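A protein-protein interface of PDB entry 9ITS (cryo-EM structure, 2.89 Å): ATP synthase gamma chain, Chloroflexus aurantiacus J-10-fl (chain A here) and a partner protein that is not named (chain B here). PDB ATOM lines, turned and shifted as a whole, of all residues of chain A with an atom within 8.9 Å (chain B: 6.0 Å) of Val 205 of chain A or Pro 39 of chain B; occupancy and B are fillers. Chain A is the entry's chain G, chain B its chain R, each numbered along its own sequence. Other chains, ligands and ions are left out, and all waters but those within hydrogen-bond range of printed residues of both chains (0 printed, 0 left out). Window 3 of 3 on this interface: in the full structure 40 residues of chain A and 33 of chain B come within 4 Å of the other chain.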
ATOM      1  N   ASN A  55      23.161 -13.551   7.159  1.00  0.00           N
ATOM      2  CA  ASN A  55      23.064 -12.177   7.642  1.00  0.00           C
ATOM      3  C   ASN A  55      23.905 -11.971   8.897  1.00  0.00           C
ATOM      4  O   ASN A  55      24.616 -10.964   9.021  1.00  0.00           O
ATOM      5  CB  ASN A  55      21.603 -11.817   7.911  1.00  0.00           C
ATOM      6  CG  ASN A  55      20.753 -11.864   6.658  1.00  0.00           C
ATOM      7  OD1 ASN A  55      21.225 -11.563   5.562  1.00  0.00           O
ATOM      8  ND2 ASN A  55      19.490 -12.243   6.814  1.00  0.00           N
ATOM      9  N   LEU A  56      23.851 -12.924   9.829  1.00  0.00           N
ATOM     10  CA  LEU A  56      24.602 -12.789  11.073  1.00  0.00           C
ATOM     11  C   LEU A  56      26.106 -12.833  10.828  1.00  0.00           C
ATOM     12  O   LEU A  56      26.860 -12.064  11.434  1.00  0.00           O
ATOM     13  CB  LEU A  56      24.180 -13.881  12.054  1.00  0.00           C
ATOM     14  CG  LEU A  56      24.740 -13.803  13.473  1.00  0.00           C
ATOM     15  CD1 LEU A  56      24.648 -12.387  14.014  1.00  0.00           C
ATOM     16  CD2 LEU A  56      23.989 -14.765  14.373  1.00  0.00           C
ATOM     17  N   ALA A  58      27.633 -12.010   8.003  1.00  0.00           N
ATOM     18  CA  ALA A  58      27.996 -10.755   7.359  1.00  0.00           C
ATOM     19  C   ALA A  58      28.030  -9.609   8.360  1.00  0.00           C
ATOM     20  O   ALA A  58      28.783  -8.646   8.172  1.00  0.00           O
ATOM     21  CB  ALA A  58      27.024 -10.445   6.221  1.00  0.00           C
ATOM     22  N   ARG A  59      27.226  -9.690   9.423  1.00  0.00           N
ATOM     23  CA  ARG A  59      27.237  -8.646  10.442  1.00  0.00           C
ATOM     24  C   ARG A  59      28.542  -8.648  11.230  1.00  0.00           C
ATOM     25  O   ARG A  59      29.165  -7.597  11.418  1.00  0.00           O
ATOM     26  CB  ARG A  59      26.044  -8.818  11.381  1.00  0.00           C
ATOM     27  CG  ARG A  59      26.008  -7.810  12.519  1.00  0.00           C
ATOM     28  CD  ARG A  59      25.865  -6.398  11.987  1.00  0.00           C
ATOM     29  NE  ARG A  59      24.644  -6.238  11.207  1.00  0.00           N
ATOM     30  CZ  ARG A  59      24.403  -5.218  10.396  1.00  0.00           C
ATOM     31  NH1 ARG A  59      25.277  -4.236  10.240  1.00  0.00           N
ATOM     32  NH2 ARG A  59      23.258  -5.182   9.721  1.00  0.00           N
ATOM     33  N   THR A 201      25.917 -10.483  -1.045  1.00  0.00           N
ATOM     34  CA  THR A 201      25.313  -9.160  -0.993  1.00  0.00           C
ATOM     35  C   THR A 201      25.118  -8.726   0.461  1.00  0.00           C
ATOM     36  O   THR A 201      25.651  -9.332   1.394  1.00  0.00           O
ATOM     37  CB  THR A 201      24.005  -9.152  -1.786  1.00  0.00           C
ATOM     38  OG1 THR A 201      23.495  -7.814  -1.865  1.00  0.00           O
ATOM     39  CG2 THR A 201      22.973 -10.062  -1.140  1.00  0.00           C
ATOM     40  N   THR A 202      24.349  -7.656   0.664  1.00  0.00           N
ATOM     41  CA  THR A 202      24.185  -7.040   1.976  1.00  0.00           C
ATOM     42  C   THR A 202      22.745  -7.155   2.466  1.00  0.00           C
ATOM     43  O   THR A 202      22.155  -6.160   2.899  1.00  0.00           O
ATOM     44  CB  THR A 202      24.611  -5.571   1.939  1.00  0.00           C
ATOM     45  OG1 THR A 202      23.800  -4.861   0.994  1.00  0.00           O
ATOM     46  CG2 THR A 202      26.073  -5.451   1.537  1.00  0.00           C
ATOM     47  N   THR A 203      22.171  -8.360   2.375  1.00  0.00           N
ATOM     48  CA  THR A 203      20.773  -8.572   2.748  1.00  0.00           C
ATOM     49  C   THR A 203      20.489  -8.159   4.189  1.00  0.00           C
ATOM     50  O   THR A 203      19.364  -7.754   4.505  1.00  0.00           O
ATOM     51  CB  THR A 203      20.393 -10.041   2.545  1.00  0.00           C
ATOM     52  OG1 THR A 203      20.949 -10.516   1.314  1.00  0.00           O
ATOM     53  CG2 THR A 203      18.881 -10.205   2.498  1.00  0.00           C
ATOM     54  N   ASN A 204      21.482  -8.245   5.072  1.00  0.00           N
ATOM     55  CA  ASN A 204      21.276  -7.862   6.462  1.00  0.00           C
ATOM     56  C   ASN A 204      21.067  -6.357   6.583  1.00  0.00           C
ATOM     57  O   ASN A 204      21.850  -5.563   6.053  1.00  0.00           O
ATOM     58  CB  ASN A 204      22.461  -8.309   7.321  1.00  0.00           C
ATOM     59  CG  ASN A 204      23.803  -7.912   6.729  1.00  0.00           C
ATOM     60  OD1 ASN A 204      23.878  -7.352   5.635  1.00  0.00           O
ATOM     61  ND2 ASN A 204      24.873  -8.193   7.462  1.00  0.00           N
ATOM     62  N   VAL A 205      19.998  -5.962   7.271  1.00  0.00           N
ATOM     63  CA  VAL A 205      19.694  -4.552   7.515  1.00  0.00           C
ATOM     64  C   VAL A 205      19.408  -4.371   9.008  1.00  0.00           C
ATOM     65  O   VAL A 205      18.272  -4.507   9.473  1.00  0.00           O
ATOM     66  CB  VAL A 205      18.553  -4.032   6.625  1.00  0.00           C
ATOM     67  CG1 VAL A 205      17.276  -4.891   6.716  1.00  0.00           C
ATOM     68  CG2 VAL A 205      18.253  -2.565   6.935  1.00  0.00           C
ATOM     69  N   ASP A 206      20.462  -4.070   9.771  1.00  0.00           N
ATOM     70  CA  ASP A 206      20.378  -3.583  11.152  1.00  0.00           C
ATOM     71  C   ASP A 206      19.480  -4.453  12.033  1.00  0.00           C
ATOM     72  O   ASP A 206      18.454  -4.009  12.552  1.00  0.00           O
ATOM     73  CB  ASP A 206      19.910  -2.127  11.175  1.00  0.00           C
ATOM     74  CG  ASP A 206      20.674  -1.258  10.196  1.00  0.00           C
ATOM     75  OD1 ASP A 206      21.801  -1.640   9.816  1.00  0.00           O
ATOM     76  OD2 ASP A 206      20.149  -0.194   9.807  1.00  0.00           O
ATOM     77  N   TYR A 207      19.874  -5.712  12.204  1.00  0.00           N
ATOM     78  CA  TYR A 207      19.136  -6.605  13.088  1.00  0.00           C
ATOM     79  C   TYR A 207      19.544  -6.359  14.535  1.00  0.00           C
ATOM     80  O   TYR A 207      20.717  -6.510  14.892  1.00  0.00           O
ATOM     81  CB  TYR A 207      19.373  -8.063  12.703  1.00  0.00           C
ATOM     82  CG  TYR A 207      18.830  -8.433  11.345  1.00  0.00           C
ATOM     83  CD1 TYR A 207      17.462  -8.526  11.129  1.00  0.00           C
ATOM     84  CD2 TYR A 207      19.680  -8.695  10.282  1.00  0.00           C
ATOM     85  CE1 TYR A 207      16.955  -8.865   9.892  1.00  0.00           C
ATOM     86  CE2 TYR A 207      19.183  -9.037   9.040  1.00  0.00           C
ATOM     87  CZ  TYR A 207      17.820  -9.119   8.850  1.00  0.00           C
ATOM     88  OH  TYR A 207      17.321  -9.458   7.614  1.00  0.00           O
ATOM     89  N   THR A 208      18.576  -5.984  15.366  1.00  0.00           N
ATOM     90  CA  THR A 208      18.828  -5.763  16.783  1.00  0.00           C
ATOM     91  C   THR A 208      18.837  -7.104  17.504  1.00  0.00           C
ATOM     92  O   THR A 208      17.860  -7.857  17.442  1.00  0.00           O
ATOM     93  CB  THR A 208      17.773  -4.835  17.380  1.00  0.00           C
ATOM     94  OG1 THR A 208      17.789  -3.581  16.686  1.00  0.00           O
ATOM     95  CG2 THR A 208      18.048  -4.595  18.855  1.00  0.00           C
ATOM     96  N   TYR A 209      19.939  -7.402  18.184  1.00  0.00           N
ATOM     97  CA  TYR A 209      20.127  -8.688  18.847  1.00  0.00           C
ATOM     98  C   TYR A 209      19.700  -8.544  20.303  1.00  0.00           C
ATOM     99  O   TYR A 209      20.385  -7.888  21.093  1.00  0.00           O
ATOM    100  CB  TYR A 209      21.581  -9.131  18.724  1.00  0.00           C
ATOM    101  CG  TYR A 209      22.053  -9.210  17.288  1.00  0.00           C
ATOM    102  CD1 TYR A 209      21.191  -9.614  16.281  1.00  0.00           C
ATOM    103  CD2 TYR A 209      23.344  -8.850  16.935  1.00  0.00           C
ATOM    104  CE1 TYR A 209      21.603  -9.683  14.969  1.00  0.00           C
ATOM    105  CE2 TYR A 209      23.768  -8.913  15.620  1.00  0.00           C
ATOM    106  CZ  TYR A 209      22.891  -9.331  14.643  1.00  0.00           C
ATOM    107  OH  TYR A 209      23.297  -9.398  13.331  1.00  0.00           O
ATOM    108  N   GLU A 210      18.557  -9.151  20.654  1.00  0.00           N
ATOM    109  CA  GLU A 210      18.001  -8.946  21.992  1.00  0.00           C
ATOM    110  C   GLU A 210      18.915  -9.476  23.094  1.00  0.00           C
ATOM    111  O   GLU A 210      19.186  -8.725  24.048  1.00  0.00           O
ATOM    112  CB  GLU A 210      16.589  -9.538  22.069  1.00  0.00           C
ATOM    113  CG  GLU A 210      15.491  -8.612  21.579  1.00  0.00           C
ATOM    114  CD  GLU A 210      15.129  -7.548  22.592  1.00  0.00           C
ATOM    115  OE1 GLU A 210      15.365  -7.768  23.799  1.00  0.00           O
ATOM    116  OE2 GLU A 210      14.603  -6.492  22.184  1.00  0.00           O
ATOM    117  N   HIS B  37       7.335  -3.491  12.844  1.00  0.00           N
ATOM    118  CA  HIS B  37       8.420  -3.598  13.814  1.00  0.00           C
ATOM    119  C   HIS B  37       9.787  -3.541  13.140  1.00  0.00           C
ATOM    120  O   HIS B  37       9.962  -3.952  11.990  1.00  0.00           O
ATOM    121  CB  HIS B  37       8.283  -4.899  14.608  1.00  0.00           C
ATOM    122  CG  HIS B  37       9.221  -5.010  15.770  1.00  0.00           C
ATOM    123  ND1 HIS B  37      10.539  -5.388  15.630  1.00  0.00           N
ATOM    124  CD2 HIS B  37       9.029  -4.804  17.094  1.00  0.00           C
ATOM    125  CE1 HIS B  37      11.120  -5.403  16.816  1.00  0.00           C
ATOM    126  NE2 HIS B  37      10.225  -5.053  17.721  1.00  0.00           N
ATOM    127  N   ALA B  38      10.763  -3.011  13.880  1.00  0.00           N
ATOM    128  CA  ALA B  38      12.131  -2.920  13.404  1.00  0.00           C
ATOM    129  C   ALA B  38      12.745  -4.315  13.284  1.00  0.00           C
ATOM    130  O   ALA B  38      12.260  -5.268  13.899  1.00  0.00           O
ATOM    131  CB  ALA B  38      12.957  -2.055  14.357  1.00  0.00           C
ATOM    132  N   PRO B  39      13.795  -4.464  12.471  1.00  0.00           N
ATOM    133  CA  PRO B  39      14.484  -5.760  12.390  1.00  0.00           C
ATOM    134  C   PRO B  39      15.025  -6.190  13.746  1.00  0.00           C
ATOM    135  O   PRO B  39      15.504  -5.373  14.534  1.00  0.00           O
ATOM    136  CB  PRO B  39      15.616  -5.499  11.391  1.00  0.00           C
ATOM    137  CG  PRO B  39      15.161  -4.348  10.583  1.00  0.00           C
ATOM    138  CD  PRO B  39      14.283  -3.511  11.458  1.00  0.00           C
ATOM    139  N   LEU B  40      14.945  -7.492  14.011  1.00  0.00           N
ATOM    140  CA  LEU B  40      15.254  -8.006  15.338  1.00  0.00           C
ATOM    141  C   LEU B  40      15.660  -9.470  15.236  1.00  0.00           C
ATOM    142  O   LEU B  40      15.196 -10.197  14.356  1.00  0.00           O
ATOM    143  CB  LEU B  40      14.048  -7.852  16.273  1.00  0.00           C
ATOM    144  CG  LEU B  40      14.240  -8.075  17.772  1.00  0.00           C
ATOM    145  CD1 LEU B  40      14.829  -6.838  18.420  1.00  0.00           C
ATOM    146  CD2 LEU B  40      12.917  -8.441  18.421  1.00  0.00           C
ATOM    147  N   MET B  41      16.530  -9.889  16.150  1.00  0.00           N
ATOM    148  CA  MET B  41      16.880 -11.290  16.329  1.00  0.00           C
ATOM    149  C   MET B  41      16.574 -11.687  17.765  1.00  0.00           C
ATOM    150  O   MET B  41      16.845 -10.928  18.700  1.00  0.00           O
ATOM    151  CB  MET B  41      18.349 -11.552  16.005  1.00  0.00           C
ATOM    152  CG  MET B  41      18.616 -12.917  15.397  1.00  0.00           C
ATOM    153  SD  MET B  41      17.891 -13.101  13.757  1.00  0.00           S
ATOM    154  CE  MET B  41      18.976 -12.055  12.788  1.00  0.00           C
ATOM    155  N   VAL B  69      12.891 -10.931  12.785  1.00  0.00           N
ATOM    156  CA  VAL B  69      11.854  -9.954  12.484  1.00  0.00           C
ATOM    157  C   VAL B  69      12.405  -9.001  11.437  1.00  0.00           C
ATOM    158  O   VAL B  69      13.366  -8.264  11.692  1.00  0.00           O
ATOM    159  CB  VAL B  69      11.400  -9.197  13.739  1.00  0.00           C
ATOM    160  CG1 VAL B  69      10.438  -8.086  13.362  1.00  0.00           C
ATOM    161  CG2 VAL B  69      10.754 -10.154  14.726  1.00  0.00           C
ATOM    162  N   LEU B  70      11.800  -9.016  10.266  1.00  0.00           N
ATOM    163  CA  LEU B  70      12.092  -8.139   9.150  1.00  0.00           C
ATOM    164  C   LEU B  70      10.949  -7.145   8.991  1.00  0.00           C
ATOM    165  O   LEU B  70       9.814  -7.433   9.381  1.00  0.00           O
ATOM    166  CB  LEU B  70      12.277  -8.975   7.873  1.00  0.00           C
ATOM    167  CG  LEU B  70      12.862  -8.419   6.572  1.00  0.00           C
ATOM    168  CD1 LEU B  70      14.321  -8.034   6.767  1.00  0.00           C
ATOM    169  CD2 LEU B  70      12.742  -9.433   5.452  1.00  0.00           C
ATOM    170  N   PRO B  71      11.210  -5.945   8.456  1.00  0.00           N
ATOM    171  CA  PRO B  71      10.146  -4.928   8.362  1.00  0.00           C
ATOM    172  C   PRO B  71       8.892  -5.357   7.608  1.00  0.00           C
ATOM    173  O   PRO B  71       7.873  -4.663   7.716  1.00  0.00           O
ATOM    174  CB  PRO B  71      10.844  -3.766   7.649  1.00  0.00           C
ATOM    175  CG  PRO B  71      12.248  -3.867   8.110  1.00  0.00           C
ATOM    176  CD  PRO B  71      12.542  -5.342   8.266  1.00  0.00           C
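O of Thr 208 of chain A is in hydrogen-bond range of N of Met 41 of chain B (2.8 Å).
The backbone NH (N) of Thr 208 of chain A lies within hydrogen-bond range of the backbone carbonyl oxygen (O) of Pro 39 of chain B (3.2 Å).
The backbone NH (N) of Glu 210 of chain A sits at hydrogen-bond distance from the backbone carbonyl oxygen (O) of Met 41 of chain B (3.1 Å).
Val 205 of chain A touches one residue of chain B.
Of chain A, only Val 205 (3.3 Å), Asp 206 (3.4 Å), Tyr 207 (3.6 Å) and Thr 208 (3.2 Å) come within 4 Å of Pro 39 of chain B.
Printed residues of chain B within 4 Å of Tyr 207 of chain A: Pro 39, Leu 40, Met 41 and Leu 70.
Printed residues of chain A within 4 Å of Met 41 of chain B: Tyr 207 (3.9 Å), Thr 208 (2.8 Å), Tyr 209 (3.5 Å) and Glu 210 (3.1 Å).
Printed residues of chain B within 4 Å of Glu 210 of chain A: Leu 40 (3.7 Å) and Met 41 (3.1 Å).
Printed residues of chain B within 4 Å of Tyr 209 of chain A: Met 41.
Printed residues of chain A within 4 Å of Leu 70 of chain B: Tyr 207 (3.4 Å).
N of Val 69 of chain B lies within hydrogen-bond range of O of Leu 40 of chain B, at 2.9 Å.
OD1 of Asp 206 of chain A is in salt-bridge range of NH2 of Arg 59 of chain A (3.8 Å).
Hydrophobic or aromatic side chains of chain B within 4 Å of the printed part of chain A: Pro 39, Leu 40, Met 41 and Leu 70.
Of the 14 printed residues of chain A, 6 touch a printed residue of chain B.
Hydrophobic or aromatic side chains of chain A within 4 Å of the printed part of chain B: Tyr 207 and Tyr 209.
Among the printed residues, 12 pairs touch across the chains.
Among the printed residues, no Asp or Glu carboxylate lies within 4 Å of a Lys or Arg side-chain nitrogen of the other chain.
Among the printed residues, merely in contact across the chains: Val 205 of chain A with Pro 39 of chain B, Asp 206 of chain A with Pro 39 of chain B, Tyr 207 of chain A with Pro 39 of chain B, Tyr 207 of chain A with Leu 40 of chain B, Tyr 207 of chain A with Met 41 of chain B, Tyr 207 of chain A with Leu 70 of chain B, Thr 208 of chain A with Leu 40 of chain B, Tyr 209 of chain A with Met 41 of chain B and Glu 210 of chain A with Leu 40 of chain B.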
